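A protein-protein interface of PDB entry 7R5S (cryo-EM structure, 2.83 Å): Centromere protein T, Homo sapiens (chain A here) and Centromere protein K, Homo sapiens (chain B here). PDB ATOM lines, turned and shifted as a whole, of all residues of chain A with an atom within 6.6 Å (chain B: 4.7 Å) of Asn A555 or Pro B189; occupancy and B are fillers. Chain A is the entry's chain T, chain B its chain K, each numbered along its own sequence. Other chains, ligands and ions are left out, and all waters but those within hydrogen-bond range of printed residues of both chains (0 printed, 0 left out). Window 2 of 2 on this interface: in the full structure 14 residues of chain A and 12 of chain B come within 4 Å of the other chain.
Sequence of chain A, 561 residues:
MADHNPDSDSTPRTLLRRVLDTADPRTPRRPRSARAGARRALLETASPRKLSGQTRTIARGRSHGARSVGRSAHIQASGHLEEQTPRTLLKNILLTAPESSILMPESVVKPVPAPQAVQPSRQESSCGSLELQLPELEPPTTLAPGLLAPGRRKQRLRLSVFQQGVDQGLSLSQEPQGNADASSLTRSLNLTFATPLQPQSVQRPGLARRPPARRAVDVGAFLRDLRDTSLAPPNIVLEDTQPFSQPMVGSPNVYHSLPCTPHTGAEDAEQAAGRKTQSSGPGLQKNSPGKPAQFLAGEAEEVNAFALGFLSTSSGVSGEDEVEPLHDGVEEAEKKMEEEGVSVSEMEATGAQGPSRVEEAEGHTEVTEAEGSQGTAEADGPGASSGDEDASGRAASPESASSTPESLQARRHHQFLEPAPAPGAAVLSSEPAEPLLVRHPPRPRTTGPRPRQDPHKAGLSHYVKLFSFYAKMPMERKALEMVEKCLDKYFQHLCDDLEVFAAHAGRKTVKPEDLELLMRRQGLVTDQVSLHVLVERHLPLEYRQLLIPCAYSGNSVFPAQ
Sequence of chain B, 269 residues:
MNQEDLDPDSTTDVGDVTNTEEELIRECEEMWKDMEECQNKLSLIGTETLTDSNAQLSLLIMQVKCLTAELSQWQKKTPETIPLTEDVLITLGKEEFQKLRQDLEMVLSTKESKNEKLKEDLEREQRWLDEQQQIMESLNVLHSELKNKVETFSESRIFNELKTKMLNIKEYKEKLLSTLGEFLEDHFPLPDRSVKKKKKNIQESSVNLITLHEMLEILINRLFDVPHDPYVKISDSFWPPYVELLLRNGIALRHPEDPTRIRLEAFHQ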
ATOM      1  N   ALA A 551      15.956  -8.916  19.103  1.00  0.00           N
ATOM      2  CA  ALA A 551      16.212 -10.331  18.885  1.00  0.00           C
ATOM      3  C   ALA A 551      14.982 -11.012  18.302  1.00  0.00           C
ATOM      4  O   ALA A 551      13.843 -10.674  18.639  1.00  0.00           O
ATOM      5  CB  ALA A 551      16.618 -11.027  20.187  1.00  0.00           C
ATOM      6  N   TYR A 552      15.228 -11.983  17.428  1.00  0.00           N
ATOM      7  CA  TYR A 552      14.163 -12.726  16.767  1.00  0.00           C
ATOM      8  C   TYR A 552      14.762 -13.955  16.100  1.00  0.00           C
ATOM      9  O   TYR A 552      15.965 -14.008  15.820  1.00  0.00           O
ATOM     10  CB  TYR A 552      13.428 -11.864  15.735  1.00  0.00           C
ATOM     11  CG  TYR A 552      14.341 -11.190  14.735  1.00  0.00           C
ATOM     12  CD1 TYR A 552      14.859  -9.925  14.979  1.00  0.00           C
ATOM     13  CD2 TYR A 552      14.684 -11.818  13.545  1.00  0.00           C
ATOM     14  CE1 TYR A 552      15.693  -9.306  14.069  1.00  0.00           C
ATOM     15  CE2 TYR A 552      15.517 -11.207  12.629  1.00  0.00           C
ATOM     16  CZ  TYR A 552      16.019  -9.951  12.895  1.00  0.00           C
ATOM     17  OH  TYR A 552      16.850  -9.340  11.984  1.00  0.00           O
ATOM     18  N   SER A 553      13.903 -14.946  15.861  1.00  0.00           N
ATOM     19  CA  SER A 553      14.222 -16.129  15.063  1.00  0.00           C
ATOM     20  C   SER A 553      15.474 -16.841  15.576  1.00  0.00           C
ATOM     21  O   SER A 553      16.501 -16.927  14.900  1.00  0.00           O
ATOM     22  CB  SER A 553      14.368 -15.758  13.585  1.00  0.00           C
ATOM     23  OG  SER A 553      13.130 -15.328  13.045  1.00  0.00           O
ATOM     24  N   GLY A 554      15.372 -17.355  16.798  1.00  0.00           N
ATOM     25  CA  GLY A 554      16.459 -18.120  17.377  1.00  0.00           C
ATOM     26  C   GLY A 554      17.543 -17.253  17.982  1.00  0.00           C
ATOM     27  O   GLY A 554      18.734 -17.502  17.771  1.00  0.00           O
ATOM     28  N   ASN A 555      17.133 -16.223  18.725  1.00  0.00           N
ATOM     29  CA  ASN A 555      18.049 -15.313  19.413  1.00  0.00           C
ATOM     30  C   ASN A 555      18.949 -14.556  18.438  1.00  0.00           C
ATOM     31  O   ASN A 555      20.037 -14.106  18.805  1.00  0.00           O
ATOM     32  CB  ASN A 555      18.894 -16.053  20.455  1.00  0.00           C
ATOM     33  CG  ASN A 555      18.050 -16.830  21.444  1.00  0.00           C
ATOM     34  OD1 ASN A 555      17.816 -18.027  21.272  1.00  0.00           O
ATOM     35  ND2 ASN A 555      17.585 -16.153  22.486  1.00  0.00           N
ATOM     36  N   SER A 556      18.509 -14.411  17.190  1.00  0.00           N
ATOM     37  CA  SER A 556      19.244 -13.612  16.217  1.00  0.00           C
ATOM     38  C   SER A 556      19.032 -12.137  16.533  1.00  0.00           C
ATOM     39  O   SER A 556      17.909 -11.634  16.432  1.00  0.00           O
ATOM     40  CB  SER A 556      18.782 -13.938  14.798  1.00  0.00           C
ATOM     41  OG  SER A 556      19.730 -13.499  13.841  1.00  0.00           O
ATOM     42  N   VAL A 557      20.101 -11.451  16.930  1.00  0.00           N
ATOM     43  CA  VAL A 557      20.030 -10.073  17.401  1.00  0.00           C
ATOM     44  C   VAL A 557      20.562  -9.154  16.310  1.00  0.00           C
ATOM     45  O   VAL A 557      21.623  -9.416  15.729  1.00  0.00           O
ATOM     46  CB  VAL A 557      20.807  -9.889  18.717  1.00  0.00           C
ATOM     47  CG1 VAL A 557      22.177 -10.548  18.629  1.00  0.00           C
ATOM     48  CG2 VAL A 557      20.937  -8.414  19.066  1.00  0.00           C
ATOM     49  N   LEU B 184       6.831 -21.089  21.286  1.00  0.00           N
ATOM     50  CA  LEU B 184       7.808 -20.313  22.043  1.00  0.00           C
ATOM     51  C   LEU B 184       9.008 -21.157  22.448  1.00  0.00           C
ATOM     52  O   LEU B 184      10.112 -20.625  22.609  1.00  0.00           O
ATOM     53  CB  LEU B 184       7.151 -19.702  23.280  1.00  0.00           C
ATOM     54  CG  LEU B 184       6.509 -18.326  23.097  1.00  0.00           C
ATOM     55  CD1 LEU B 184       5.884 -17.853  24.398  1.00  0.00           C
ATOM     56  CD2 LEU B 184       7.535 -17.324  22.597  1.00  0.00           C
ATOM     57  N   GLU B 185       8.819 -22.467  22.618  1.00  0.00           N
ATOM     58  CA  GLU B 185       9.944 -23.321  22.977  1.00  0.00           C
ATOM     59  C   GLU B 185      10.829 -23.622  21.774  1.00  0.00           C
ATOM     60  O   GLU B 185      12.059 -23.580  21.883  1.00  0.00           O
ATOM     61  CB  GLU B 185       9.438 -24.620  23.605  1.00  0.00           C
ATOM     62  CG  GLU B 185      10.502 -25.698  23.748  1.00  0.00           C
ATOM     63  CD  GLU B 185      11.671 -25.260  24.609  1.00  0.00           C
ATOM     64  OE1 GLU B 185      11.454 -24.481  25.562  1.00  0.00           O
ATOM     65  OE2 GLU B 185      12.809 -25.693  24.332  1.00  0.00           O
ATOM     66  N   HIS B 187      11.045 -21.937  18.865  1.00  0.00           N
ATOM     67  CA  HIS B 187      11.526 -20.775  18.126  1.00  0.00           C
ATOM     68  C   HIS B 187      12.408 -19.847  18.948  1.00  0.00           C
ATOM     69  O   HIS B 187      13.272 -19.172  18.378  1.00  0.00           O
ATOM     70  CB  HIS B 187      10.343 -19.976  17.567  1.00  0.00           C
ATOM     71  CG  HIS B 187      10.015 -20.302  16.144  1.00  0.00           C
ATOM     72  ND1 HIS B 187      10.443 -19.531  15.086  1.00  0.00           N
ATOM     73  CD2 HIS B 187       9.304 -21.320  15.604  1.00  0.00           C
ATOM     74  CE1 HIS B 187      10.006 -20.057  13.956  1.00  0.00           C
ATOM     75  NE2 HIS B 187       9.312 -21.143  14.242  1.00  0.00           N
ATOM     76  N   PHE B 188      12.223 -19.791  20.266  1.00  0.00           N
ATOM     77  CA  PHE B 188      12.990 -18.904  21.141  1.00  0.00           C
ATOM     78  C   PHE B 188      13.559 -19.717  22.295  1.00  0.00           C
ATOM     79  O   PHE B 188      13.000 -19.729  23.400  1.00  0.00           O
ATOM     80  CB  PHE B 188      12.128 -17.750  21.653  1.00  0.00           C
ATOM     81  CG  PHE B 188      11.813 -16.719  20.608  1.00  0.00           C
ATOM     82  CD1 PHE B 188      10.724 -16.874  19.767  1.00  0.00           C
ATOM     83  CD2 PHE B 188      12.606 -15.593  20.467  1.00  0.00           C
ATOM     84  CE1 PHE B 188      10.433 -15.927  18.805  1.00  0.00           C
ATOM     85  CE2 PHE B 188      12.320 -14.642  19.507  1.00  0.00           C
ATOM     86  CZ  PHE B 188      11.231 -14.809  18.676  1.00  0.00           C
ATOM     87  N   PRO B 189      14.681 -20.409  22.077  1.00  0.00           N
ATOM     88  CA  PRO B 189      15.289 -21.192  23.161  1.00  0.00           C
ATOM     89  C   PRO B 189      15.910 -20.313  24.235  1.00  0.00           C
ATOM     90  O   PRO B 189      15.825 -19.082  24.171  1.00  0.00           O
ATOM     91  CB  PRO B 189      16.355 -22.030  22.439  1.00  0.00           C
ATOM     92  CG  PRO B 189      16.024 -21.927  20.974  1.00  0.00           C
ATOM     93  CD  PRO B 189      15.394 -20.587  20.804  1.00  0.00           C
ATOM     94  N   LEU B 190      16.535 -20.935  25.225  1.00  0.00           N
ATOM     95  CA  LEU B 190      17.188 -20.180  26.287  1.00  0.00           C
ATOM     96  C   LEU B 190      18.414 -19.461  25.732  1.00  0.00           C
ATOM     97  O   LEU B 190      19.291 -20.106  25.145  1.00  0.00           O
ATOM     98  CB  LEU B 190      17.592 -21.109  27.430  1.00  0.00           C
ATOM     99  CG  LEU B 190      18.271 -20.462  28.639  1.00  0.00           C
ATOM    100  CD1 LEU B 190      17.313 -19.531  29.366  1.00  0.00           C
ATOM    101  CD2 LEU B 190      18.812 -21.524  29.583  1.00  0.00           C
ATOM    102  N   PRO B 191      18.513 -18.144  25.891  1.00  0.00           N
ATOM    103  CA  PRO B 191      19.678 -17.427  25.364  1.00  0.00           C
ATOM    104  C   PRO B 191      20.927 -17.711  26.180  1.00  0.00           C
ATOM    105  O   PRO B 191      20.879 -17.890  27.399  1.00  0.00           O
ATOM    106  CB  PRO B 191      19.266 -15.955  25.472  1.00  0.00           C
ATOM    107  CG  PRO B 191      18.288 -15.932  26.598  1.00  0.00           C
ATOM    108  CD  PRO B 191      17.539 -17.234  26.519  1.00  0.00           C
ATOM    109  N   THR B 211      13.607 -17.150  30.189  1.00  0.00           N
ATOM    110  CA  THR B 211      13.064 -17.212  28.842  1.00  0.00           C
ATOM    111  C   THR B 211      11.943 -16.190  28.663  1.00  0.00           C
ATOM    112  O   THR B 211      11.478 -15.554  29.613  1.00  0.00           O
ATOM    113  CB  THR B 211      12.549 -18.619  28.537  1.00  0.00           C
ATOM    114  OG1 THR B 211      11.760 -19.089  29.637  1.00  0.00           O
ATOM    115  CG2 THR B 211      13.710 -19.573  28.308  1.00  0.00           C
ATOM    116  N   TRP B 239      16.365  -9.067  29.615  1.00  0.00           N
ATOM    117  CA  TRP B 239      17.414  -8.387  28.874  1.00  0.00           C
ATOM    118  C   TRP B 239      16.815  -7.538  27.751  1.00  0.00           C
ATOM    119  O   TRP B 239      15.704  -7.808  27.286  1.00  0.00           O
ATOM    120  CB  TRP B 239      18.425  -9.394  28.320  1.00  0.00           C
ATOM    121  CG  TRP B 239      17.954 -10.256  27.188  1.00  0.00           C
ATOM    122  CD1 TRP B 239      16.673 -10.637  26.916  1.00  0.00           C
ATOM    123  CD2 TRP B 239      18.775 -10.858  26.179  1.00  0.00           C
ATOM    124  NE1 TRP B 239      16.645 -11.432  25.796  1.00  0.00           N
ATOM    125  CE2 TRP B 239      17.922 -11.584  25.325  1.00  0.00           C
ATOM    126  CE3 TRP B 239      20.147 -10.850  25.913  1.00  0.00           C
ATOM    127  CZ2 TRP B 239      18.397 -12.294  24.224  1.00  0.00           C
ATOM    128  CZ3 TRP B 239      20.616 -11.557  24.820  1.00  0.00           C
ATOM    129  CH2 TRP B 239      19.743 -12.269  23.989  1.00  0.00           C
ATOM    130  N   TYR B 242      14.560  -8.961  24.460  1.00  0.00           N
ATOM    131  CA  TYR B 242      13.180  -9.429  24.571  1.00  0.00           C
ATOM    132  C   TYR B 242      12.231  -8.288  24.917  1.00  0.00           C
ATOM    133  O   TYR B 242      11.102  -8.235  24.411  1.00  0.00           O
ATOM    134  CB  TYR B 242      13.080 -10.542  25.614  1.00  0.00           C
ATOM    135  CG  TYR B 242      13.667 -11.861  25.166  1.00  0.00           C
ATOM    136  CD1 TYR B 242      14.024 -12.072  23.841  1.00  0.00           C
ATOM    137  CD2 TYR B 242      13.862 -12.898  26.069  1.00  0.00           C
ATOM    138  CE1 TYR B 242      14.561 -13.276  23.429  1.00  0.00           C
ATOM    139  CE2 TYR B 242      14.400 -14.105  25.666  1.00  0.00           C
ATOM    140  CZ  TYR B 242      14.747 -14.289  24.344  1.00  0.00           C
ATOM    141  OH  TYR B 242      15.281 -15.490  23.939  1.00  0.00           O
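N of Gly A554 is in hydrogen-bond range of O of His B187. ND2 of Asn A555 is in hydrogen-bond range of OH of Tyr B242.
Among the printed residues, pairs that only touch across the chains: Tyr A552 with Phe B188, Ser A553 with Phe B188, Asn A555 with Pro B189 and Asn A555 with Pro B191.
Asn A555 touches just these residues of chain B: Pro B189 (3.6 Å), Pro B191 (3.4 Å) and Tyr B242 (2.8 Å). Pro B189 touches one residue of chain A. Of the printed residues of chain A, Tyr B242 touches Asn A555. Printed residues of chain B within 4 Å of Ser A553: Phe B188. Ser A556 touches none of the printed residues of chain B. The nearest residue of chain B that does not touch Asn A555 is Trp B239 (4.3 Å). The nearest printed residue of chain B that does not touch Ser A553 is His B187 (4.3 Å).
Of the 10 printed residues of chain B, 5 touch a printed residue of chain A. Among the printed residues, 6 pairs touch across the chains. Among the printed residues, no Asp or Glu carboxylate lies within 4 Å of a Lys or Arg side-chain nitrogen of the other chain.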
